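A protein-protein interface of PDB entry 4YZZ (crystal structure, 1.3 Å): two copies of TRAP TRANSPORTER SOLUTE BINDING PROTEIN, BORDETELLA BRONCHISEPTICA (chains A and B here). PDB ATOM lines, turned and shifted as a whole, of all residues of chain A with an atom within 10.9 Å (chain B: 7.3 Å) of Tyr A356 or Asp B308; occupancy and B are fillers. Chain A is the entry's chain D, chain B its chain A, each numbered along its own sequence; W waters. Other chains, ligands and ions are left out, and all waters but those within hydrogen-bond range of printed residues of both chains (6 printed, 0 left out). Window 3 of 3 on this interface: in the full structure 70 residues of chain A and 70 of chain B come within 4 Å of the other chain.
Of the 18 printed residues of chain B, 8 touch a printed residue of chain A.
Water W4 lies within hydrogen-bond range of the side-chain amide oxygen of Asn B351 (2.5 Å) and the side-chain carboxylate of Asp A354 (2.9 Å).
Water W3 lies within hydrogen-bond range of OD1 of Asn B351 and ND2 of Asn A351.
Water W5 lies within hydrogen-bond range of the side-chain carboxylate of Asp A354 (2.7 Å), the side-chain amide oxygen of Asn A351 (3.1 Å) and the side-chain amide nitrogen of Asn B351 (3.2 Å).
Water W6 bridges O of Ala A360 (2.7 Å) and OH of Tyr B311 (2.8 Å).
Water W1 bridges the backbone carbonyl oxygen of Ala A359 and the guanidinium group of Arg B347.
Water W2 lies within hydrogen-bond range of O of Asn A355 (2.8 Å) and NE of Arg B347 (3.1 Å).
Of the printed residues of chain B, Tyr A356 touches Phe B117, Met B307, Asp B308 and Tyr B311.
Asp B308 touches just one residue of chain A: Tyr A356 (2.6 Å).
No residue of chain A comes within 4 Å of Glu B305.
No residue of chain A comes within 4 Å of Val B306.
Met B307 touches just one residue of chain A: Tyr A356 (3.5 Å).
No residue of chain A comes within 4 Å of Val B310.
No residue of chain A comes within 4 Å of Lys B312.
Printed residues of chain A within 4 Å of Arg B347: Ala A359 and Ala A362.
Of the printed residues of chain B, Asn A355 touches Asn B351 (3.0 Å).
Val A361 touches none of the printed residues of chain B.
Pro B303 touches none of the printed residues of chain A.
The nearest residue of chain B that does not touch Tyr A356 is Lys B304 (5.1 Å).
N of Phe B117 sits at hydrogen-bond distance from O of Trp B239, at 3.0 Å.
The backbone carbonyl oxygen of Phe A346 is in hydrogen-bond range of the backbone NH of Asn A351, 2.9 Å away.
OD2 of Asp B308 is in salt-bridge range of NZ of Lys B304, 2.9 Å away.
The backbone carbonyl oxygen (O) of Asn A351 lies within hydrogen-bond range of the side-chain amide nitrogen (ND2) of Asn A355.
OG1 of Thr A357 is in hydrogen-bond range of O of Leu A353, 3.3 Å away.
The side-chain amide nitrogen (ND2) of Asn B351 sits at hydrogen-bond distance from the side-chain amide oxygen (OD1) of Asn A355 (3.0 Å).
OD1 of Asp B308 is in hydrogen-bond range of OH of Tyr A356.
Among the printed residues, pairs that only touch across the chains: Ala A349 with Pro B237 (3.8 Å), Asn A351 with Asn B351 (3.8 Å), Leu A353 with Phe B117 (3.9 Å), Leu A353 with Pro B237 (3.9 Å), Leu A353 with Trp B239 (3.9 Å), Asp A354 with Asn B351 (3.8 Å), Tyr A356 with Phe B117 (3.6 Å), Tyr A356 with Met B307 (3.5 Å), Tyr A356 with Tyr B311 (3.6 Å), Thr A357 with Phe B117 (3.4 Å), Phe A358 with Asn B351 (3.3 Å), Ala A359 with Arg B347 (3.8 Å), Ala A360 with Tyr B311 (3.7 Å), Ala A362 with Arg B347 (3.7 Å) and Ala A364 with Tyr B311 (3.9999 Å).
Asn B351 touches its own counterpart, Asn A351.
Positions printed for both chains: 347 and 351.
Of the 17 pairs that touch across the chains among the printed residues, 1 has its exchanged pair printed and touching as well.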
ATOM      1  N   PHE A 346      21.471  12.986 -41.681  1.00  0.00           N
ATOM      2  CA  PHE A 346      22.621  12.796 -40.798  1.00  0.00           C
ATOM      3  C   PHE A 346      22.532  13.705 -39.572  1.00  0.00           C
ATOM      4  O   PHE A 346      23.078  13.370 -38.526  1.00  0.00           O
ATOM      5  CB  PHE A 346      23.950  13.007 -41.550  1.00  0.00           C
ATOM      6  CG  PHE A 346      24.471  11.766 -42.268  1.00  0.00           C
ATOM      7  CD1 PHE A 346      23.740  11.149 -43.264  1.00  0.00           C
ATOM      8  CD2 PHE A 346      25.727  11.267 -41.973  1.00  0.00           C
ATOM      9  CE1 PHE A 346      24.234  10.042 -43.932  1.00  0.00           C
ATOM     10  CE2 PHE A 346      26.227  10.157 -42.651  1.00  0.00           C
ATOM     11  CZ  PHE A 346      25.478   9.551 -43.630  1.00  0.00           C
ATOM     12  N   ARG A 347      21.873  14.857 -39.699  1.00  0.00           N
ATOM     13  CA  ARG A 347      21.674  15.755 -38.563  1.00  0.00           C
ATOM     14  C   ARG A 347      20.806  15.133 -37.479  1.00  0.00           C
ATOM     15  O   ARG A 347      20.938  15.499 -36.301  1.00  0.00           O
ATOM     16  CB  ARG A 347      21.072  17.087 -39.008  1.00  0.00           C
ATOM     17  CG  ARG A 347      22.121  17.987 -39.655  1.00  0.00           C
ATOM     18  CD  ARG A 347      21.738  19.443 -39.742  1.00  0.00           C
ATOM     19  NE  ARG A 347      20.692  19.672 -40.727  1.00  0.00           N
ATOM     20  CZ  ARG A 347      19.408  19.855 -40.443  1.00  0.00           C
ATOM     21  NH1 ARG A 347      18.975  19.840 -39.185  1.00  0.00           N
ATOM     22  NH2 ARG A 347      18.549  20.054 -41.434  1.00  0.00           N
ATOM     23  N   VAL A 348      19.908  14.222 -37.850  1.00  0.00           N
ATOM     24  CA  VAL A 348      18.924  13.683 -36.928  1.00  0.00           C
ATOM     25  C   VAL A 348      19.527  12.697 -35.939  1.00  0.00           C
ATOM     26  O   VAL A 348      19.201  12.748 -34.752  1.00  0.00           O
ATOM     27  CB  VAL A 348      17.766  13.004 -37.687  1.00  0.00           C
ATOM     28  CG1 VAL A 348      16.814  12.303 -36.732  1.00  0.00           C
ATOM     29  CG2 VAL A 348      17.008  14.018 -38.518  1.00  0.00           C
ATOM     30  N   ALA A 349      20.341  11.758 -36.411  1.00  0.00           N
ATOM     31  CA  ALA A 349      20.873  10.718 -35.538  1.00  0.00           C
ATOM     32  C   ALA A 349      22.390  10.645 -35.572  1.00  0.00           C
ATOM     33  O   ALA A 349      23.036  10.743 -34.536  1.00  0.00           O
ATOM     34  CB  ALA A 349      20.236   9.351 -35.859  1.00  0.00           C
ATOM     35  N   GLU A 350      22.968  10.480 -36.757  1.00  0.00           N
ATOM     36  CA  GLU A 350      24.405  10.255 -36.888  1.00  0.00           C
ATOM     37  C   GLU A 350      25.229  11.342 -36.179  1.00  0.00           C
ATOM     38  O   GLU A 350      26.043  11.068 -35.294  1.00  0.00           O
ATOM     39  CB  GLU A 350      24.774  10.158 -38.378  1.00  0.00           C
ATOM     40  CG  GLU A 350      26.045   9.394 -38.647  1.00  0.00           C
ATOM     41  CD  GLU A 350      25.953   7.892 -38.407  1.00  0.00           C
ATOM     42  OE1 GLU A 350      24.919   7.243 -38.686  1.00  0.00           O
ATOM     43  OE2 GLU A 350      26.984   7.359 -37.988  1.00  0.00           O
ATOM     44  N   ASN A 351      25.007  12.594 -36.553  1.00  0.00           N
ATOM     45  CA  ASN A 351      25.798  13.677 -35.974  1.00  0.00           C
ATOM     46  C   ASN A 351      25.367  14.063 -34.575  1.00  0.00           C
ATOM     47  O   ASN A 351      26.196  14.494 -33.767  1.00  0.00           O
ATOM     48  CB  ASN A 351      25.791  14.886 -36.896  1.00  0.00           C
ATOM     49  CG  ASN A 351      26.756  14.726 -38.022  1.00  0.00           C
ATOM     50  OD1 ASN A 351      26.637  13.791 -38.806  1.00  0.00           O
ATOM     51  ND2 ASN A 351      27.753  15.605 -38.091  1.00  0.00           N
ATOM     52  N   ALA A 352      24.097  13.830 -34.271  1.00  0.00           N
ATOM     53  CA  ALA A 352      23.612  14.017 -32.911  1.00  0.00           C
ATOM     54  C   ALA A 352      24.416  13.144 -31.954  1.00  0.00           C
ATOM     55  O   ALA A 352      24.910  13.617 -30.937  1.00  0.00           O
ATOM     56  CB  ALA A 352      22.136  13.692 -32.833  1.00  0.00           C
ATOM     57  N   LEU A 353      24.582  11.870 -32.289  1.00  0.00           N
ATOM     58  CA  LEU A 353      25.319  10.987 -31.405  1.00  0.00           C
ATOM     59  C   LEU A 353      26.819  11.260 -31.433  1.00  0.00           C
ATOM     60  O   LEU A 353      27.442  11.369 -30.381  1.00  0.00           O
ATOM     61  CB  LEU A 353      25.042   9.516 -31.732  1.00  0.00           C
ATOM     62  CG  LEU A 353      25.689   8.550 -30.742  1.00  0.00           C
ATOM     63  CD1 LEU A 353      25.245   8.783 -29.308  1.00  0.00           C
ATOM     64  CD2 LEU A 353      25.404   7.103 -31.155  1.00  0.00           C
ATOM     65  N   ASP A 354      27.398  11.404 -32.617  1.00  0.00           N
ATOM     66  CA  ASP A 354      28.844  11.619 -32.688  1.00  0.00           C
ATOM     67  C   ASP A 354      29.248  12.903 -31.950  1.00  0.00           C
ATOM     68  O   ASP A 354      30.230  12.915 -31.209  1.00  0.00           O
ATOM     69  CB  ASP A 354      29.323  11.692 -34.133  1.00  0.00           C
ATOM     70  CG  ASP A 354      29.579  10.322 -34.765  1.00  0.00           C
ATOM     71  OD1 ASP A 354      29.571   9.300 -34.043  1.00  0.00           O
ATOM     72  OD2 ASP A 354      29.815  10.314 -36.010  1.00  0.00           O
ATOM     73  N   ASN A 355      28.471  13.975 -32.110  1.00  0.00           N
ATOM     74  CA  ASN A 355      28.836  15.214 -31.439  1.00  0.00           C
ATOM     75  C   ASN A 355      28.799  15.022 -29.923  1.00  0.00           C
ATOM     76  O   ASN A 355      29.663  15.539 -29.210  1.00  0.00           O
ATOM     77  CB  ASN A 355      27.947  16.377 -31.875  1.00  0.00           C
ATOM     78  CG  ASN A 355      28.236  16.841 -33.286  1.00  0.00           C
ATOM     79  OD1 ASN A 355      29.343  16.684 -33.801  1.00  0.00           O
ATOM     80  ND2 ASN A 355      27.236  17.439 -33.913  1.00  0.00           N
ATOM     81  N   TYR A 356      27.821  14.262 -29.424  1.00  0.00           N
ATOM     82  CA  TYR A 356      27.724  13.997 -27.993  1.00  0.00           C
ATOM     83  C   TYR A 356      28.913  13.153 -27.527  1.00  0.00           C
ATOM     84  O   TYR A 356      29.610  13.490 -26.575  1.00  0.00           O
ATOM     85  CB  TYR A 356      26.396  13.305 -27.654  1.00  0.00           C
ATOM     86  CG  TYR A 356      26.218  13.115 -26.171  1.00  0.00           C
ATOM     87  CD1 TYR A 356      26.867  12.094 -25.502  1.00  0.00           C
ATOM     88  CD2 TYR A 356      25.446  13.994 -25.419  1.00  0.00           C
ATOM     89  CE1 TYR A 356      26.723  11.931 -24.134  1.00  0.00           C
ATOM     90  CE2 TYR A 356      25.303  13.831 -24.052  1.00  0.00           C
ATOM     91  CZ  TYR A 356      25.969  12.821 -23.421  1.00  0.00           C
ATOM     92  OH  TYR A 356      25.846  12.640 -22.066  1.00  0.00           O
ATOM     93  N   THR A 357      29.138  12.050 -28.220  1.00  0.00           N
ATOM     94  CA  THR A 357      30.169  11.106 -27.814  1.00  0.00           C
ATOM     95  C   THR A 357      31.567  11.715 -27.843  1.00  0.00           C
ATOM     96  O   THR A 357      32.354  11.540 -26.916  1.00  0.00           O
ATOM     97  CB  THR A 357      30.111   9.845 -28.684  1.00  0.00           C
ATOM     98  OG1 THR A 357      28.904   9.152 -28.375  1.00  0.00           O
ATOM     99  CG2 THR A 357      31.307   8.913 -28.430  1.00  0.00           C
ATOM    100  N   PHE A 358      31.891  12.433 -28.906  1.00  0.00           N
ATOM    101  CA  PHE A 358      33.252  12.965 -29.037  1.00  0.00           C
ATOM    102  C   PHE A 358      33.527  13.935 -27.901  1.00  0.00           C
ATOM    103  O   PHE A 358      34.625  13.948 -27.330  1.00  0.00           O
ATOM    104  CB  PHE A 358      33.480  13.684 -30.371  1.00  0.00           C
ATOM    105  CG  PHE A 358      33.326  12.814 -31.594  1.00  0.00           C
ATOM    106  CD1 PHE A 358      33.289  11.427 -31.520  1.00  0.00           C
ATOM    107  CD2 PHE A 358      33.248  13.404 -32.850  1.00  0.00           C
ATOM    108  CE1 PHE A 358      33.147  10.653 -32.669  1.00  0.00           C
ATOM    109  CE2 PHE A 358      33.124  12.637 -33.988  1.00  0.00           C
ATOM    110  CZ  PHE A 358      33.077  11.265 -33.911  1.00  0.00           C
ATOM    111  N   ALA A 359      32.525  14.724 -27.534  1.00  0.00           N
ATOM    112  CA  ALA A 359      32.687  15.651 -26.415  1.00  0.00           C
ATOM    113  C   ALA A 359      32.818  14.903 -25.083  1.00  0.00           C
ATOM    114  O   ALA A 359      33.637  15.260 -24.228  1.00  0.00           O
ATOM    115  CB  ALA A 359      31.526  16.629 -26.355  1.00  0.00           C
ATOM    116  N   ALA A 360      32.025  13.852 -24.901  1.00  0.00           N
ATOM    117  CA  ALA A 360      32.086  13.073 -23.661  1.00  0.00           C
ATOM    118  C   ALA A 360      33.417  12.336 -23.503  1.00  0.00           C
ATOM    119  O   ALA A 360      33.983  12.276 -22.399  1.00  0.00           O
ATOM    120  CB  ALA A 360      30.936  12.082 -23.591  1.00  0.00           C
ATOM    121  N   VAL A 361      33.901  11.767 -24.603  1.00  0.00           N
ATOM    122  CA  VAL A 361      35.157  11.023 -24.598  1.00  0.00           C
ATOM    123  C   VAL A 361      36.293  11.949 -24.190  1.00  0.00           C
ATOM    124  O   VAL A 361      37.173  11.569 -23.421  1.00  0.00           O
ATOM    125  CB  VAL A 361      35.429  10.365 -25.974  1.00  0.00           C
ATOM    126  CG1 VAL A 361      36.861   9.869 -26.088  1.00  0.00           C
ATOM    127  CG2 VAL A 361      34.461   9.204 -26.201  1.00  0.00           C
ATOM    128  N   ALA A 362      36.258  13.173 -24.694  1.00  0.00           N
ATOM    129  CA  ALA A 362      37.271  14.160 -24.336  1.00  0.00           C
ATOM    130  C   ALA A 362      37.247  14.497 -22.845  1.00  0.00           C
ATOM    131  O   ALA A 362      38.296  14.641 -22.204  1.00  0.00           O
ATOM    132  CB  ALA A 362      37.076  15.422 -25.165  1.00  0.00           C
ATOM    133  N   ARG A 363      36.050  14.644 -22.285  1.00  0.00           N
ATOM    134  CA  ARG A 363      35.920  14.951 -20.865  1.00  0.00           C
ATOM    135  C   ARG A 363      36.445  13.812 -20.001  1.00  0.00           C
ATOM    136  O   ARG A 363      37.070  14.049 -18.970  1.00  0.00           O
ATOM    137  CB  ARG A 363      34.460  15.250 -20.496  1.00  0.00           C
ATOM    138  CG  ARG A 363      33.880  16.499 -21.145  1.00  0.00           C
ATOM    139  CD  ARG A 363      32.536  16.910 -20.518  1.00  0.00           C
ATOM    140  NE  ARG A 363      31.490  15.892 -20.657  1.00  0.00           N
ATOM    141  CZ  ARG A 363      30.637  15.804 -21.680  1.00  0.00           C
ATOM    142  NH1 ARG A 363      30.690  16.663 -22.681  1.00  0.00           N
ATOM    143  NH2 ARG A 363      29.720  14.847 -21.700  1.00  0.00           N
ATOM    144  N   ALA A 364      36.190  12.575 -20.411  1.00  0.00           N
ATOM    145  CA  ALA A 364      36.611  11.429 -19.619  1.00  0.00           C
ATOM    146  C   ALA A 364      38.123  11.221 -19.692  1.00  0.00           C
ATOM    147  O   ALA A 364      38.733  10.703 -18.752  1.00  0.00           O
ATOM    148  CB  ALA A 364      35.884  10.197 -20.081  1.00  0.00           C
ATOM    149  N   PHE B 117      27.531   4.402 -26.819  1.00  0.00           N
ATOM    150  CA  PHE B 117      28.391   5.572 -26.966  1.00  0.00           C
ATOM    151  C   PHE B 117      29.788   5.183 -27.455  1.00  0.00           C
ATOM    152  O   PHE B 117      30.796   5.800 -27.106  1.00  0.00           O
ATOM    153  CB  PHE B 117      28.463   6.374 -25.661  1.00  0.00           C
ATOM    154  CG  PHE B 117      27.143   6.995 -25.258  1.00  0.00           C
ATOM    155  CD1 PHE B 117      26.738   8.207 -25.799  1.00  0.00           C
ATOM    156  CD2 PHE B 117      26.300   6.355 -24.351  1.00  0.00           C
ATOM    157  CE1 PHE B 117      25.516   8.782 -25.419  1.00  0.00           C
ATOM    158  CE2 PHE B 117      25.092   6.929 -23.975  1.00  0.00           C
ATOM    159  CZ  PHE B 117      24.703   8.137 -24.502  1.00  0.00           C
ATOM    160  N   THR B 169      14.264  10.737 -17.136  1.00  0.00           N
ATOM    161  CA  THR B 169      14.469   9.326 -16.829  1.00  0.00           C
ATOM    162  C   THR B 169      13.279   8.706 -16.084  1.00  0.00           C
ATOM    163  O   THR B 169      13.130   7.491 -16.071  1.00  0.00           O
ATOM    164  CB  THR B 169      15.769   9.099 -16.044  1.00  0.00           C
ATOM    165  OG1 THR B 169      15.672   9.764 -14.787  1.00  0.00           O
ATOM    166  CG2 THR B 169      16.969   9.641 -16.800  1.00  0.00           C
ATOM    167  N   PRO B 237      19.097  10.221 -30.527  1.00  0.00           N
ATOM    168  CA  PRO B 237      19.697   9.123 -31.286  1.00  0.00           C
ATOM    169  C   PRO B 237      19.692   7.818 -30.519  1.00  0.00           C
ATOM    170  O   PRO B 237      19.572   7.802 -29.300  1.00  0.00           O
ATOM    171  CB  PRO B 237      21.136   9.602 -31.472  1.00  0.00           C
ATOM    172  CG  PRO B 237      21.431  10.260 -30.179  1.00  0.00           C
ATOM    173  CD  PRO B 237      20.132  10.962 -29.778  1.00  0.00           C
ATOM    174  N   TRP B 239      21.776   5.783 -28.980  1.00  0.00           N
ATOM    175  CA  TRP B 239      23.070   5.714 -28.319  1.00  0.00           C
ATOM    176  C   TRP B 239      23.517   4.282 -28.018  1.00  0.00           C
ATOM    177  O   TRP B 239      24.680   4.046 -27.649  1.00  0.00           O
ATOM    178  CB  TRP B 239      23.022   6.548 -27.024  1.00  0.00           C
ATOM    179  CG  TRP B 239      21.897   6.113 -26.139  1.00  0.00           C
ATOM    180  CD1 TRP B 239      20.652   6.672 -26.050  1.00  0.00           C
ATOM    181  CD2 TRP B 239      21.901   5.006 -25.238  1.00  0.00           C
ATOM    182  NE1 TRP B 239      19.889   5.966 -25.176  1.00  0.00           N
ATOM    183  CE2 TRP B 239      20.632   4.934 -24.662  1.00  0.00           C
ATOM    184  CE3 TRP B 239      22.858   4.050 -24.885  1.00  0.00           C
ATOM    185  CZ2 TRP B 239      20.289   3.957 -23.744  1.00  0.00           C
ATOM    186  CZ3 TRP B 239      22.523   3.095 -23.984  1.00  0.00           C
ATOM    187  CH2 TRP B 239      21.254   3.043 -23.420  1.00  0.00           C
ATOM    188  N   PRO B 303      16.023  14.214 -24.387  1.00  0.00           N
ATOM    189  CA  PRO B 303      16.544  15.328 -23.596  1.00  0.00           C
ATOM    190  C   PRO B 303      17.982  15.114 -23.144  1.00  0.00           C
ATOM    191  O   PRO B 303      18.413  13.983 -22.937  1.00  0.00           O
ATOM    192  CB  PRO B 303      15.607  15.367 -22.382  1.00  0.00           C
ATOM    193  CG  PRO B 303      14.359  14.715 -22.845  1.00  0.00           C
ATOM    194  CD  PRO B 303      14.786  13.659 -23.809  1.00  0.00           C
ATOM    195  N   LYS B 304      18.713  16.207 -22.972  1.00  0.00           N
ATOM    196  CA  LYS B 304      20.100  16.140 -22.536  1.00  0.00           C
ATOM    197  C   LYS B 304      20.243  15.346 -21.249  1.00  0.00           C
ATOM    198  O   LYS B 304      21.186  14.570 -21.101  1.00  0.00           O
ATOM    199  CB  LYS B 304      20.663  17.551 -22.353  1.00  0.00           C
ATOM    200  CG  LYS B 304      22.069  17.618 -21.785  1.00  0.00           C
ATOM    201  CD  LYS B 304      22.488  19.084 -21.612  1.00  0.00           C
ATOM    202  CE  LYS B 304      23.924  19.223 -21.119  1.00  0.00           C
ATOM    203  NZ  LYS B 304      24.137  18.524 -19.809  1.00  0.00           N
ATOM    204  N   GLU B 305      19.302  15.516 -20.323  1.00  0.00           N
ATOM    205  CA  GLU B 305      19.387  14.833 -19.037  1.00  0.00           C
ATOM    206  C   GLU B 305      19.249  13.326 -19.210  1.00  0.00           C
ATOM    207  O   GLU B 305      19.871  12.558 -18.478  1.00  0.00           O
ATOM    208  CB  GLU B 305      18.309  15.356 -18.075  1.00  0.00           C
ATOM    209  CG  GLU B 305      18.497  16.794 -17.685  1.00  0.00           C
ATOM    210  CD  GLU B 305      17.992  17.775 -18.721  1.00  0.00           C
ATOM    211  OE1 GLU B 305      17.265  17.367 -19.653  1.00  0.00           O
ATOM    212  OE2 GLU B 305      18.325  18.973 -18.592  1.00  0.00           O
ATOM    213  N   VAL B 306      18.448  12.897 -20.178  1.00  0.00           N
ATOM    214  CA  VAL B 306      18.314  11.474 -20.449  1.00  0.00           C
ATOM    215  C   VAL B 306      19.604  10.935 -21.082  1.00  0.00           C
ATOM    216  O   VAL B 306      20.112   9.888 -20.679  1.00  0.00           O
ATOM    217  CB  VAL B 306      17.099  11.191 -21.336  1.00  0.00           C
ATOM    218  CG1 VAL B 306      17.125   9.759 -21.856  1.00  0.00           C
ATOM    219  CG2 VAL B 306      15.811  11.464 -20.572  1.00  0.00           C
ATOM    220  N   MET B 307      20.152  11.674 -22.044  1.00  0.00           N
ATOM    221  CA  MET B 307      21.433  11.314 -22.643  1.00  0.00           C
ATOM    222  C   MET B 307      22.517  11.182 -21.583  1.00  0.00           C
ATOM    223  O   MET B 307      23.288  10.239 -21.583  1.00  0.00           O
ATOM    224  CB  MET B 307      21.852  12.365 -23.683  1.00  0.00           C
ATOM    225  CG  MET B 307      20.956  12.374 -24.909  1.00  0.00           C
ATOM    226  SD  MET B 307      21.096  10.908 -25.943  1.00  0.00           S
ATOM    227  CE  MET B 307      22.749  11.083 -26.598  1.00  0.00           C
ATOM    228  N   ASP B 308      22.600  12.150 -20.690  1.00  0.00           N
ATOM    229  CA  ASP B 308      23.623  12.107 -19.649  1.00  0.00           C
ATOM    230  C   ASP B 308      23.457  10.894 -18.723  1.00  0.00           C
ATOM    231  O   ASP B 308      24.431  10.269 -18.309  1.00  0.00           O
ATOM    232  CB  ASP B 308      23.593  13.398 -18.810  1.00  0.00           C
ATOM    233  CG  ASP B 308      24.024  14.640 -19.589  1.00  0.00           C
ATOM    234  OD1 ASP B 308      24.623  14.528 -20.679  1.00  0.00           O
ATOM    235  OD2 ASP B 308      23.773  15.760 -19.081  1.00  0.00           O
ATOM    236  N   ALA B 309      22.217  10.552 -18.407  1.00  0.00           N
ATOM    237  CA  ALA B 309      21.941   9.444 -17.512  1.00  0.00           C
ATOM    238  C   ALA B 309      22.353   8.129 -18.149  1.00  0.00           C
ATOM    239  O   ALA B 309      22.962   7.287 -17.497  1.00  0.00           O
ATOM    240  CB  ALA B 309      20.464   9.408 -17.156  1.00  0.00           C
ATOM    241  N   VAL B 310      22.007   7.927 -19.415  1.00  0.00           N
ATOM    242  CA  VAL B 310      22.381   6.679 -20.053  1.00  0.00           C
ATOM    243  C   VAL B 310      23.889   6.630 -20.326  1.00  0.00           C
ATOM    244  O   VAL B 310      24.498   5.544 -20.309  1.00  0.00           O
ATOM    245  CB  VAL B 310      21.543   6.369 -21.312  1.00  0.00           C
ATOM    246  CG1 VAL B 310      20.084   6.141 -20.910  1.00  0.00           C
ATOM    247  CG2 VAL B 310      21.671   7.454 -22.367  1.00  0.00           C
ATOM    248  N   TYR B 311      24.516   7.777 -20.607  1.00  0.00           N
ATOM    249  CA  TYR B 311      25.967   7.804 -20.741  1.00  0.00           C
ATOM    250  C   TYR B 311      26.648   7.327 -19.447  1.00  0.00           C
ATOM    251  O   TYR B 311      27.540   6.466 -19.472  1.00  0.00           O
ATOM    252  CB  TYR B 311      26.471   9.190 -21.157  1.00  0.00           C
ATOM    253  CG  TYR B 311      27.982   9.230 -21.165  1.00  0.00           C
ATOM    254  CD1 TYR B 311      28.699   8.766 -22.255  1.00  0.00           C
ATOM    255  CD2 TYR B 311      28.683   9.676 -20.049  1.00  0.00           C
ATOM    256  CE1 TYR B 311      30.096   8.758 -22.232  1.00  0.00           C
ATOM    257  CE2 TYR B 311      30.041   9.688 -20.015  1.00  0.00           C
ATOM    258  CZ  TYR B 311      30.749   9.237 -21.106  1.00  0.00           C
ATOM    259  OH  TYR B 311      32.117   9.247 -21.033  1.00  0.00           O
ATOM    260  N   LYS B 312      26.228   7.890 -18.320  1.00  0.00           N
ATOM    261  CA  LYS B 312      26.803   7.516 -17.029  1.00  0.00           C
ATOM    262  C   LYS B 312      26.558   6.044 -16.707  1.00  0.00           C
ATOM    263  O   LYS B 312      27.450   5.354 -16.204  1.00  0.00           O
ATOM    264  CB  LYS B 312      26.266   8.421 -15.916  1.00  0.00           C
ATOM    265  CG  LYS B 312      26.827   9.822 -15.950  1.00  0.00           C
ATOM    266  CD  LYS B 312      26.406  10.591 -14.688  1.00  0.00           C
ATOM    267  CE  LYS B 312      25.282  11.559 -14.948  1.00  0.00           C
ATOM    268  NZ  LYS B 312      25.821  12.834 -15.501  1.00  0.00           N
ATOM    269  N   ALA B 313      25.355   5.555 -16.997  1.00  0.00           N
ATOM    270  CA  ALA B 313      25.053   4.146 -16.778  1.00  0.00           C
ATOM    271  C   ALA B 313      25.946   3.245 -17.642  1.00  0.00           C
ATOM    272  O   ALA B 313      26.394   2.190 -17.190  1.00  0.00           O
ATOM    273  CB  ALA B 313      23.574   3.880 -17.039  1.00  0.00           C
ATOM    274  N   SER B 314      26.218   3.683 -18.871  1.00  0.00           N
ATOM    275  CA  SER B 314      27.085   2.952 -19.782  1.00  0.00           C
ATOM    276  C   SER B 314      28.491   2.822 -19.190  1.00  0.00           C
ATOM    277  O   SER B 314      29.079   1.738 -19.181  1.00  0.00           O
ATOM    278  CB  SER B 314      27.179   3.674 -21.130  1.00  0.00           C
ATOM    279  OG  SER B 314      25.979   3.597 -21.867  1.00  0.00           O
ATOM    280  N   ARG B 347      36.684  14.894 -34.309  1.00  0.00           N
ATOM    281  CA  ARG B 347      36.185  16.162 -33.835  1.00  0.00           C
ATOM    282  C   ARG B 347      36.873  17.323 -34.543  1.00  0.00           C
ATOM    283  O   ARG B 347      36.242  18.348 -34.811  1.00  0.00           O
ATOM    284  CB  ARG B 347      36.399  16.258 -32.326  1.00  0.00           C
ATOM    285  CG  ARG B 347      35.559  17.307 -31.670  1.00  0.00           C
ATOM    286  CD  ARG B 347      35.779  17.289 -30.170  1.00  0.00           C
ATOM    287  NE  ARG B 347      34.802  18.127 -29.483  1.00  0.00           N
ATOM    288  CZ  ARG B 347      34.870  18.462 -28.198  1.00  0.00           C
ATOM    289  NH1 ARG B 347      35.874  18.034 -27.441  1.00  0.00           N
ATOM    290  NH2 ARG B 347      33.931  19.234 -27.671  1.00  0.00           N
ATOM    291  N   ASN B 351      34.046  15.994 -38.359  1.00  0.00           N
ATOM    292  CA  ASN B 351      32.869  16.615 -37.779  1.00  0.00           C
ATOM    293  C   ASN B 351      32.881  18.114 -37.846  1.00  0.00           C
ATOM    294  O   ASN B 351      31.821  18.727 -37.941  1.00  0.00           O
ATOM    295  CB  ASN B 351      32.639  16.116 -36.366  1.00  0.00           C
ATOM    296  CG  ASN B 351      31.898  14.848 -36.384  1.00  0.00           C
ATOM    297  OD1 ASN B 351      32.360  13.888 -37.000  1.00  0.00           O
ATOM    298  ND2 ASN B 351      30.697  14.835 -35.798  1.00  0.00           N
HETATM  299  O   HOH W   1      34.698  17.762 -24.302  1.00  0.00           O
HETATM  300  O   HOH W   2      31.912  17.050 -30.076  1.00  0.00           O
HETATM  301  O   HOH W   3      30.595  14.037 -38.930  1.00  0.00           O
HETATM  302  O   HOH W   4      31.965  11.496 -37.495  1.00  0.00           O
HETATM  303  O   HOH W   5      28.955  12.530 -37.199  1.00  0.00           O
HETATM  304  O   HOH W   6      32.807  11.736 -20.071  1.00  0.00           O
